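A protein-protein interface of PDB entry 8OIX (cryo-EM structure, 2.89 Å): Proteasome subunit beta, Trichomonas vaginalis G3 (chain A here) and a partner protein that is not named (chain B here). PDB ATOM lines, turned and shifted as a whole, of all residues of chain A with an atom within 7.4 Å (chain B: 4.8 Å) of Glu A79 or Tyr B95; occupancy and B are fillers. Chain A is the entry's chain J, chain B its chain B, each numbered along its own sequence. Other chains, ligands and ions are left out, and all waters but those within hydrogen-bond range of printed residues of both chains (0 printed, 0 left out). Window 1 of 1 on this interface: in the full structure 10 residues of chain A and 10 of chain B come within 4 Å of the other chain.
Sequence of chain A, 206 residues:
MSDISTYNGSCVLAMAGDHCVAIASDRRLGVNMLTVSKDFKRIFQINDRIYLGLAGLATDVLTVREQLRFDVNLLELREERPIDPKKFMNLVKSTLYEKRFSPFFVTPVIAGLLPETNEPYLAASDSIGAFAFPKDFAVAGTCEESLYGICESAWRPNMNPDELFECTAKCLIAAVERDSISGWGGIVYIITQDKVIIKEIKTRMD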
ATOM      1  N   ASN A  73     -34.060  19.503  15.151  1.00  0.00           N
ATOM      2  CA  ASN A  73     -34.413  19.545  16.562  1.00  0.00           C
ATOM      3  C   ASN A  73     -33.484  18.670  17.392  1.00  0.00           C
ATOM      4  O   ASN A  73     -33.047  19.081  18.471  1.00  0.00           O
ATOM      5  CB  ASN A  73     -35.868  19.132  16.753  1.00  0.00           C
ATOM      6  CG  ASN A  73     -36.842  20.182  16.258  1.00  0.00           C
ATOM      7  OD1 ASN A  73     -36.440  21.255  15.811  1.00  0.00           O
ATOM      8  ND2 ASN A  73     -38.131  19.876  16.334  1.00  0.00           N
ATOM      9  N   LEU A  74     -33.154  17.467  16.908  1.00  0.00           N
ATOM     10  CA  LEU A  74     -32.218  16.634  17.658  1.00  0.00           C
ATOM     11  C   LEU A  74     -30.845  17.285  17.748  1.00  0.00           C
ATOM     12  O   LEU A  74     -30.206  17.249  18.805  1.00  0.00           O
ATOM     13  CB  LEU A  74     -32.113  15.243  17.038  1.00  0.00           C
ATOM     14  CG  LEU A  74     -33.303  14.322  17.289  1.00  0.00           C
ATOM     15  CD1 LEU A  74     -33.019  12.954  16.723  1.00  0.00           C
ATOM     16  CD2 LEU A  74     -33.580  14.233  18.775  1.00  0.00           C
ATOM     17  N   LEU A  75     -30.372  17.883  16.653  1.00  0.00           N
ATOM     18  CA  LEU A  75     -29.074  18.546  16.680  1.00  0.00           C
ATOM     19  C   LEU A  75     -29.067  19.714  17.656  1.00  0.00           C
ATOM     20  O   LEU A  75     -28.107  19.897  18.410  1.00  0.00           O
ATOM     21  CB  LEU A  75     -28.695  19.014  15.277  1.00  0.00           C
ATOM     22  CG  LEU A  75     -28.194  17.907  14.354  1.00  0.00           C
ATOM     23  CD1 LEU A  75     -28.193  18.374  12.912  1.00  0.00           C
ATOM     24  CD2 LEU A  75     -26.813  17.444  14.781  1.00  0.00           C
ATOM     25  N   GLU A  76     -30.135  20.513  17.664  1.00  0.00           N
ATOM     26  CA  GLU A  76     -30.169  21.681  18.534  1.00  0.00           C
ATOM     27  C   GLU A  76     -30.366  21.291  19.993  1.00  0.00           C
ATOM     28  O   GLU A  76     -29.908  22.008  20.888  1.00  0.00           O
ATOM     29  CB  GLU A  76     -31.264  22.646  18.086  1.00  0.00           C
ATOM     30  CG  GLU A  76     -31.030  23.245  16.710  1.00  0.00           C
ATOM     31  CD  GLU A  76     -32.184  24.103  16.246  1.00  0.00           C
ATOM     32  OE1 GLU A  76     -33.127  24.310  17.039  1.00  0.00           O
ATOM     33  OE2 GLU A  76     -32.143  24.587  15.097  1.00  0.00           O
ATOM     34  N   LEU A  77     -31.045  20.175  20.254  1.00  0.00           N
ATOM     35  CA  LEU A  77     -31.137  19.676  21.621  1.00  0.00           C
ATOM     36  C   LEU A  77     -29.795  19.137  22.097  1.00  0.00           C
ATOM     37  O   LEU A  77     -29.338  19.462  23.199  1.00  0.00           O
ATOM     38  CB  LEU A  77     -32.218  18.601  21.712  1.00  0.00           C
ATOM     39  CG  LEU A  77     -33.653  19.092  21.535  1.00  0.00           C
ATOM     40  CD1 LEU A  77     -34.581  17.924  21.277  1.00  0.00           C
ATOM     41  CD2 LEU A  77     -34.099  19.874  22.755  1.00  0.00           C
ATOM     42  N   ARG A  78     -29.145  18.311  21.275  1.00  0.00           N
ATOM     43  CA  ARG A  78     -27.885  17.697  21.667  1.00  0.00           C
ATOM     44  C   ARG A  78     -26.728  18.686  21.668  1.00  0.00           C
ATOM     45  O   ARG A  78     -25.685  18.396  22.262  1.00  0.00           O
ATOM     46  CB  ARG A  78     -27.574  16.520  20.741  1.00  0.00           C
ATOM     47  CG  ARG A  78     -28.582  15.388  20.843  1.00  0.00           C
ATOM     48  CD  ARG A  78     -28.246  14.235  19.915  1.00  0.00           C
ATOM     49  NE  ARG A  78     -28.419  14.590  18.513  1.00  0.00           N
ATOM     50  CZ  ARG A  78     -28.631  13.715  17.538  1.00  0.00           C
ATOM     51  NH1 ARG A  78     -28.722  12.418  17.783  1.00  0.00           N
ATOM     52  NH2 ARG A  78     -28.759  14.152  16.290  1.00  0.00           N
ATOM     53  N   GLU A  79     -26.888  19.847  21.037  1.00  0.00           N
ATOM     54  CA  GLU A  79     -25.813  20.821  20.937  1.00  0.00           C
ATOM     55  C   GLU A  79     -26.158  22.171  21.541  1.00  0.00           C
ATOM     56  O   GLU A  79     -25.291  23.053  21.572  1.00  0.00           O
ATOM     57  CB  GLU A  79     -25.411  21.018  19.470  1.00  0.00           C
ATOM     58  CG  GLU A  79     -24.955  19.751  18.783  1.00  0.00           C
ATOM     59  CD  GLU A  79     -24.564  19.982  17.342  1.00  0.00           C
ATOM     60  OE1 GLU A  79     -24.275  21.143  16.984  1.00  0.00           O
ATOM     61  OE2 GLU A  79     -24.541  19.003  16.567  1.00  0.00           O
ATOM     62  N   GLU A  80     -27.389  22.365  22.014  1.00  0.00           N
ATOM     63  CA  GLU A  80     -27.822  23.600  22.665  1.00  0.00           C
ATOM     64  C   GLU A  80     -27.591  24.829  21.789  1.00  0.00           C
ATOM     65  O   GLU A  80     -27.550  25.955  22.293  1.00  0.00           O
ATOM     66  CB  GLU A  80     -27.129  23.782  24.020  1.00  0.00           C
ATOM     67  CG  GLU A  80     -27.260  22.591  24.959  1.00  0.00           C
ATOM     68  CD  GLU A  80     -28.526  22.629  25.796  1.00  0.00           C
ATOM     69  OE1 GLU A  80     -29.601  22.955  25.251  1.00  0.00           O
ATOM     70  OE2 GLU A  80     -28.443  22.332  27.006  1.00  0.00           O
ATOM     71  N   ARG A  81     -27.440  24.629  20.480  1.00  0.00           N
ATOM     72  CA  ARG A  81     -27.120  25.698  19.553  1.00  0.00           C
ATOM     73  C   ARG A  81     -27.961  25.547  18.293  1.00  0.00           C
ATOM     74  O   ARG A  81     -28.215  24.416  17.852  1.00  0.00           O
ATOM     75  CB  ARG A  81     -25.629  25.673  19.191  1.00  0.00           C
ATOM     76  CG  ARG A  81     -25.085  26.981  18.659  1.00  0.00           C
ATOM     77  CD  ARG A  81     -23.594  27.087  18.920  1.00  0.00           C
ATOM     78  NE  ARG A  81     -23.278  26.914  20.333  1.00  0.00           N
ATOM     79  CZ  ARG A  81     -23.527  27.810  21.280  1.00  0.00           C
ATOM     80  NH1 ARG A  81     -24.097  28.971  21.002  1.00  0.00           N
ATOM     81  NH2 ARG A  81     -23.197  27.534  22.537  1.00  0.00           N
ATOM     82  N   PRO A  82     -28.405  26.653  17.699  1.00  0.00           N
ATOM     83  CA  PRO A  82     -29.109  26.562  16.416  1.00  0.00           C
ATOM     84  C   PRO A  82     -28.189  26.044  15.321  1.00  0.00           C
ATOM     85  O   PRO A  82     -26.971  26.231  15.361  1.00  0.00           O
ATOM     86  CB  PRO A  82     -29.548  28.005  16.146  1.00  0.00           C
ATOM     87  CG  PRO A  82     -29.523  28.672  17.478  1.00  0.00           C
ATOM     88  CD  PRO A  82     -28.414  28.023  18.237  1.00  0.00           C
ATOM     89  N   ILE A  83     -28.787  25.387  14.339  1.00  0.00           N
ATOM     90  CA  ILE A  83     -28.027  24.803  13.240  1.00  0.00           C
ATOM     91  C   ILE A  83     -27.620  25.899  12.263  1.00  0.00           C
ATOM     92  O   ILE A  83     -28.375  26.847  12.012  1.00  0.00           O
ATOM     93  CB  ILE A  83     -28.842  23.690  12.554  1.00  0.00           C
ATOM     94  CG1 ILE A  83     -27.937  22.828  11.674  1.00  0.00           C
ATOM     95  CG2 ILE A  83     -30.000  24.265  11.752  1.00  0.00           C
ATOM     96  CD1 ILE A  83     -28.605  21.578  11.164  1.00  0.00           C
ATOM     97  N   ASP A  84     -26.397  25.802  11.752  1.00  0.00           N
ATOM     98  CA  ASP A  84     -25.892  26.769  10.793  1.00  0.00           C
ATOM     99  C   ASP A  84     -26.506  26.529   9.418  1.00  0.00           C
ATOM    100  O   ASP A  84     -26.950  25.420   9.110  1.00  0.00           O
ATOM    101  CB  ASP A  84     -24.372  26.679  10.708  1.00  0.00           C
ATOM    102  CG  ASP A  84     -23.709  26.727  12.067  1.00  0.00           C
ATOM    103  OD1 ASP A  84     -23.992  25.841  12.899  1.00  0.00           O
ATOM    104  OD2 ASP A  84     -22.901  27.652  12.303  1.00  0.00           O
ATOM    105  N   LYS A  87     -24.315  23.916   7.897  1.00  0.00           N
ATOM    106  CA  LYS A  87     -24.568  22.658   8.589  1.00  0.00           C
ATOM    107  C   LYS A  87     -25.912  22.078   8.180  1.00  0.00           C
ATOM    108  O   LYS A  87     -26.031  20.871   7.942  1.00  0.00           O
ATOM    109  CB  LYS A  87     -24.512  22.868  10.103  1.00  0.00           C
ATOM    110  CG  LYS A  87     -24.319  21.587  10.893  1.00  0.00           C
ATOM    111  CD  LYS A  87     -24.427  21.829  12.387  1.00  0.00           C
ATOM    112  CE  LYS A  87     -23.059  22.000  13.018  1.00  0.00           C
ATOM    113  NZ  LYS A  87     -23.151  22.341  14.462  1.00  0.00           N
ATOM    114  N   ASN A  90     -25.629  20.639   4.611  1.00  0.00           N
ATOM    115  CA  ASN A  90     -25.044  19.304   4.622  1.00  0.00           C
ATOM    116  C   ASN A  90     -26.013  18.288   5.209  1.00  0.00           C
ATOM    117  O   ASN A  90     -26.035  17.129   4.784  1.00  0.00           O
ATOM    118  CB  ASN A  90     -23.737  19.303   5.401  1.00  0.00           C
ATOM    119  CG  ASN A  90     -22.644  20.074   4.710  1.00  0.00           C
ATOM    120  OD1 ASN A  90     -21.960  19.554   3.830  1.00  0.00           O
ATOM    121  ND2 ASN A  90     -22.445  21.316   5.130  1.00  0.00           N
ATOM    122  N   ALA B  91     -16.809   8.831  14.639  1.00  0.00           N
ATOM    123  CA  ALA B  91     -17.981   9.660  14.891  1.00  0.00           C
ATOM    124  C   ALA B  91     -17.782  11.067  14.348  1.00  0.00           C
ATOM    125  O   ALA B  91     -18.718  11.670  13.819  1.00  0.00           O
ATOM    126  CB  ALA B  91     -18.284   9.701  16.387  1.00  0.00           C
ATOM    127  N   SER B  92     -16.568  11.604  14.470  1.00  0.00           N
ATOM    128  CA  SER B  92     -16.289  12.936  13.947  1.00  0.00           C
ATOM    129  C   SER B  92     -16.355  12.961  12.427  1.00  0.00           C
ATOM    130  O   SER B  92     -16.899  13.905  11.843  1.00  0.00           O
ATOM    131  CB  SER B  92     -14.923  13.417  14.432  1.00  0.00           C
ATOM    132  OG  SER B  92     -14.921  13.590  15.837  1.00  0.00           O
ATOM    133  N   ILE B  93     -15.799  11.947  11.762  1.00  0.00           N
ATOM    134  CA  ILE B  93     -15.876  11.930  10.305  1.00  0.00           C
ATOM    135  C   ILE B  93     -17.310  11.688   9.847  1.00  0.00           C
ATOM    136  O   ILE B  93     -17.734  12.228   8.820  1.00  0.00           O
ATOM    137  CB  ILE B  93     -14.883  10.917   9.694  1.00  0.00           C
ATOM    138  CG1 ILE B  93     -15.181   9.480  10.125  1.00  0.00           C
ATOM    139  CG2 ILE B  93     -13.452  11.294  10.053  1.00  0.00           C
ATOM    140  CD1 ILE B  93     -16.059   8.698   9.163  1.00  0.00           C
ATOM    141  N   LYS B  94     -18.084  10.887  10.586  1.00  0.00           N
ATOM    142  CA  LYS B  94     -19.503  10.739  10.276  1.00  0.00           C
ATOM    143  C   LYS B  94     -20.242  12.059  10.448  1.00  0.00           C
ATOM    144  O   LYS B  94     -21.119  12.402   9.647  1.00  0.00           O
ATOM    145  CB  LYS B  94     -20.126   9.661  11.163  1.00  0.00           C
ATOM    146  CG  LYS B  94     -19.899   8.243  10.677  1.00  0.00           C
ATOM    147  CD  LYS B  94     -20.582   7.243  11.593  1.00  0.00           C
ATOM    148  CE  LYS B  94     -22.082   7.487  11.646  1.00  0.00           C
ATOM    149  NZ  LYS B  94     -22.797   6.427  12.410  1.00  0.00           N
ATOM    150  N   TYR B  95     -19.914  12.803  11.506  1.00  0.00           N
ATOM    151  CA  TYR B  95     -20.514  14.111  11.727  1.00  0.00           C
ATOM    152  C   TYR B  95     -20.153  15.065  10.600  1.00  0.00           C
ATOM    153  O   TYR B  95     -20.976  15.885  10.184  1.00  0.00           O
ATOM    154  CB  TYR B  95     -20.056  14.663  13.078  1.00  0.00           C
ATOM    155  CG  TYR B  95     -20.816  15.875  13.566  1.00  0.00           C
ATOM    156  CD1 TYR B  95     -20.560  17.137  13.050  1.00  0.00           C
ATOM    157  CD2 TYR B  95     -21.779  15.757  14.557  1.00  0.00           C
ATOM    158  CE1 TYR B  95     -21.248  18.242  13.498  1.00  0.00           C
ATOM    159  CE2 TYR B  95     -22.469  16.858  15.014  1.00  0.00           C
ATOM    160  CZ  TYR B  95     -22.201  18.097  14.480  1.00  0.00           C
ATOM    161  OH  TYR B  95     -22.889  19.199  14.928  1.00  0.00           O
ATOM    162  N   SER B  96     -18.916  14.991  10.113  1.00  0.00           N
ATOM    163  CA  SER B  96     -18.513  15.801   8.969  1.00  0.00           C
ATOM    164  C   SER B  96     -19.271  15.396   7.710  1.00  0.00           C
ATOM    165  O   SER B  96     -19.669  16.254   6.916  1.00  0.00           O
ATOM    166  CB  SER B  96     -17.006  15.684   8.751  1.00  0.00           C
ATOM    167  OG  SER B  96     -16.294  16.157   9.879  1.00  0.00           O
ATOM    168  N   LEU B  97     -19.465  14.094   7.501  1.00  0.00           N
ATOM    169  CA  LEU B  97     -20.201  13.638   6.328  1.00  0.00           C
ATOM    170  C   LEU B  97     -21.647  14.111   6.368  1.00  0.00           C
ATOM    171  O   LEU B  97     -22.194  14.554   5.351  1.00  0.00           O
ATOM    172  CB  LEU B  97     -20.144  12.115   6.234  1.00  0.00           C
ATOM    173  CG  LEU B  97     -18.776  11.521   5.921  1.00  0.00           C
ATOM    174  CD1 LEU B  97     -18.829  10.004   5.940  1.00  0.00           C
ATOM    175  CD2 LEU B  97     -18.306  12.028   4.581  1.00  0.00           C
ATOM    176  N   ARG B  98     -22.282  14.022   7.534  1.00  0.00           N
ATOM    177  CA  ARG B  98     -23.683  14.395   7.660  1.00  0.00           C
ATOM    178  C   ARG B  98     -23.888  15.901   7.768  1.00  0.00           C
ATOM    179  O   ARG B  98     -24.959  16.394   7.402  1.00  0.00           O
ATOM    180  CB  ARG B  98     -24.291  13.689   8.878  1.00  0.00           C
ATOM    181  CG  ARG B  98     -25.728  14.060   9.189  1.00  0.00           C
ATOM    182  CD  ARG B  98     -26.351  13.075  10.158  1.00  0.00           C
ATOM    183  NE  ARG B  98     -27.588  13.586  10.734  1.00  0.00           N
ATOM    184  CZ  ARG B  98     -27.666  14.224  11.894  1.00  0.00           C
ATOM    185  NH1 ARG B  98     -26.593  14.450  12.631  1.00  0.00           N
ATOM    186  NH2 ARG B  98     -28.852  14.646  12.322  1.00  0.00           N
ATOM    187  N   LEU B  99     -22.881  16.646   8.226  1.00  0.00           N
ATOM    188  CA  LEU B  99     -23.058  18.054   8.553  1.00  0.00           C
ATOM    189  C   LEU B  99     -21.936  18.962   8.064  1.00  0.00           C
ATOM    190  O   LEU B  99     -22.024  20.176   8.272  1.00  0.00           O
ATOM    191  CB  LEU B  99     -23.236  18.226  10.069  1.00  0.00           C
ATOM    192  CG  LEU B  99     -24.430  17.451  10.633  1.00  0.00           C
ATOM    193  CD1 LEU B  99     -24.392  17.372  12.131  1.00  0.00           C
ATOM    194  CD2 LEU B  99     -25.726  18.088  10.174  1.00  0.00           C
ATOM    195  N   GLY B 100     -20.895  18.429   7.429  1.00  0.00           N
ATOM    196  CA  GLY B 100     -19.894  19.247   6.776  1.00  0.00           C
ATOM    197  C   GLY B 100     -18.909  19.936   7.690  1.00  0.00           C
ATOM    198  O   GLY B 100     -18.055  20.684   7.198  1.00  0.00           O
ATOM    199  N   VAL B 101     -18.992  19.714   8.999  1.00  0.00           N
ATOM    200  CA  VAL B 101     -18.092  20.337   9.956  1.00  0.00           C
ATOM    201  C   VAL B 101     -17.601  19.272  10.922  1.00  0.00           C
ATOM    202  O   VAL B 101     -18.234  18.232  11.114  1.00  0.00           O
ATOM    203  CB  VAL B 101     -18.762  21.492  10.730  1.00  0.00           C
ATOM    204  CG1 VAL B 101     -19.139  22.622   9.788  1.00  0.00           C
ATOM    205  CG2 VAL B 101     -19.980  20.986  11.475  1.00  0.00           C
ATOM    206  N   GLU B 102     -16.446  19.541  11.525  1.00  0.00           N
ATOM    207  CA  GLU B 102     -15.919  18.643  12.541  1.00  0.00           C
ATOM    208  C   GLU B 102     -16.892  18.560  13.707  1.00  0.00           C
ATOM    209  O   GLU B 102     -17.542  19.546  14.064  1.00  0.00           O
ATOM    210  CB  GLU B 102     -14.551  19.124  13.025  1.00  0.00           C
ATOM    211  CG  GLU B 102     -13.493  19.296  11.937  1.00  0.00           C
ATOM    212  CD  GLU B 102     -12.997  17.981  11.349  1.00  0.00           C
ATOM    213  OE1 GLU B 102     -13.822  17.116  10.984  1.00  0.00           O
ATOM    214  OE2 GLU B 102     -11.765  17.811  11.257  1.00  0.00           O
ATOM    215  N   MET B 103     -17.007  17.370  14.282  1.00  0.00           N
ATOM    216  CA  MET B 103     -17.914  17.169  15.401  1.00  0.00           C
ATOM    217  C   MET B 103     -17.553  18.128  16.531  1.00  0.00           C
ATOM    218  O   MET B 103     -16.378  18.206  16.915  1.00  0.00           O
ATOM    219  CB  MET B 103     -17.847  15.721  15.882  1.00  0.00           C
ATOM    220  CG  MET B 103     -18.856  15.373  16.958  1.00  0.00           C
ATOM    221  SD  MET B 103     -18.739  13.656  17.488  1.00  0.00           S
ATOM    222  CE  MET B 103     -20.290  13.007  16.878  1.00  0.00           C
ATOM    223  N   PRO B 104     -18.515  18.894  17.061  1.00  0.00           N
ATOM    224  CA  PRO B 104     -18.211  19.831  18.149  1.00  0.00           C
ATOM    225  C   PRO B 104     -17.521  19.165  19.324  1.00  0.00           C
ATOM    226  O   PRO B 104     -17.604  17.945  19.495  1.00  0.00           O
ATOM    227  CB  PRO B 104     -19.591  20.366  18.544  1.00  0.00           C
ATOM    228  CG  PRO B 104     -20.398  20.248  17.312  1.00  0.00           C
ATOM    229  CD  PRO B 104     -19.903  19.024  16.595  1.00  0.00           C
ATOM    230  N   ARG B 106     -18.134  19.365  22.615  1.00  0.00           N
ATOM    231  CA  ARG B 106     -19.069  18.726  23.530  1.00  0.00           C
ATOM    232  C   ARG B 106     -19.794  17.569  22.861  1.00  0.00           C
ATOM    233  O   ARG B 106     -20.166  16.609  23.537  1.00  0.00           O
ATOM    234  CB  ARG B 106     -20.068  19.745  24.075  1.00  0.00           C
ATOM    235  CG  ARG B 106     -21.067  19.152  25.061  1.00  0.00           C
ATOM    236  CD  ARG B 106     -21.891  20.225  25.739  1.00  0.00           C
ATOM    237  NE  ARG B 106     -22.243  21.299  24.821  1.00  0.00           N
ATOM    238  CZ  ARG B 106     -23.326  21.309  24.056  1.00  0.00           C
ATOM    239  NH1 ARG B 106     -24.191  20.308  24.072  1.00  0.00           N
ATOM    240  NH2 ARG B 106     -23.543  22.346  23.254  1.00  0.00           N
ATOM    241  N   GLU B 107     -19.976  17.616  21.541  1.00  0.00           N
ATOM    242  CA  GLU B 107     -20.545  16.465  20.846  1.00  0.00           C
ATOM    243  C   GLU B 107     -19.594  15.276  20.867  1.00  0.00           C
ATOM    244  O   GLU B 107     -20.027  14.134  21.058  1.00  0.00           O
ATOM    245  CB  GLU B 107     -20.907  16.839  19.412  1.00  0.00           C
ATOM    246  CG  GLU B 107     -22.189  17.619  19.298  1.00  0.00           C
ATOM    247  CD  GLU B 107     -23.403  16.757  19.572  1.00  0.00           C
ATOM    248  OE1 GLU B 107     -23.736  15.907  18.719  1.00  0.00           O
ATOM    249  OE2 GLU B 107     -24.017  16.917  20.645  1.00  0.00           O
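O of Leu B99 sits at hydrogen-bond distance from ND2 of Asn A90, at 3.4 Å. O of Glu A79 is in hydrogen-bond range of NH2 of Arg B106, 2.5 Å away. The side-chain carboxylate (OE1) of Glu A79 lies close to the side-chain hydroxyl (OH) of Tyr B95 (3.2 Å). The backbone carbonyl oxygen (O) of Arg A78 sits close to the side-chain carboxylate (OE2) of Glu B107, at 2.8 Å. O of Asn A90 lies close to O of Arg B98 (2.9 Å). The backbone carbonyl oxygen (O) of Arg A78 is in hydrogen-bond range of the guanidinium group (NH1) of Arg B106. The side-chain amino group (NZ) of Lys A87 is in hydrogen-bond range of the side-chain hydroxyl (OH) of Tyr B95, at 3.2 Å.
The side-chain carboxylate of Glu A79 lies within salt-bridge range of the side-chain amino group of Lys A87 (3.0 Å). The backbone carbonyl oxygen of Leu A74 lies close to the guanidinium group of Arg A78 (3.2 Å). NZ of Lys A87 lies within salt-bridge range of OD1 of Asp A84 (3.9 Å). The backbone carbonyl oxygen (O) of Val B101 sits at hydrogen-bond distance from the side-chain hydroxyl (OG) of Ser B96 (3.1 Å).
Arg B98 touches Leu A75 (NH1 to CD2, 3.7 Å). Leu A75 touches Leu B99 (CD2 to CD1, 3.6 Å). Arg A78 touches Arg B98 (NH2 to NH2, 3.9997 Å). Glu A79 touches Pro B104 (OE1 to CG, 3.99 Å). CD of Glu B107 touches CG of Glu A79, 3.5 Å away. CG of Glu A80 touches NH1 of Arg B106, at 3.9 Å. O of Leu B99 touches CA of Lys A87, at 3.6 Å. CG2 of Val B101 touches CE of Lys A87, at 3.6 Å. Gly B100 touches Asn A90.
Tyr B95 touches just these residues of chain A: Glu A79 (2.3 Å) and Lys A87 (3.2 Å). Of the printed residues of chain A, Glu B107 touches Arg A78 and Glu A79. Of the printed residues of chain B, Leu A75 touches Arg B98 (3.7 Å) and Leu B99 (3.6 Å). Glu A76 touches none of the printed residues of chain B. Asn A73 touches none of the printed residues of chain B. The nearest printed residue of chain B that does not touch Glu A79 is Leu B99 (4.7 Å).
Of the 14 printed residues of chain A, 6 touch a printed residue of chain B. Printed residues of chain A that touch a printed residue of chain B: Leu A75, Arg A78, Glu A79, Glu A80, Lys A87 and Asn A90. Hydrophobic or aromatic side chains of chain A within 4 Å of the printed part of chain B: Leu A75. Printed residues of chain B that touch a printed residue of chain A: Tyr B95, Arg B98, Leu B99, Gly B100, Val B101, Pro B104, Arg B106 and Glu B107. Among the printed residues, no Asp or Glu carboxylate lies within 4 Å of a Lys or Arg side-chain nitrogen of the other chain.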
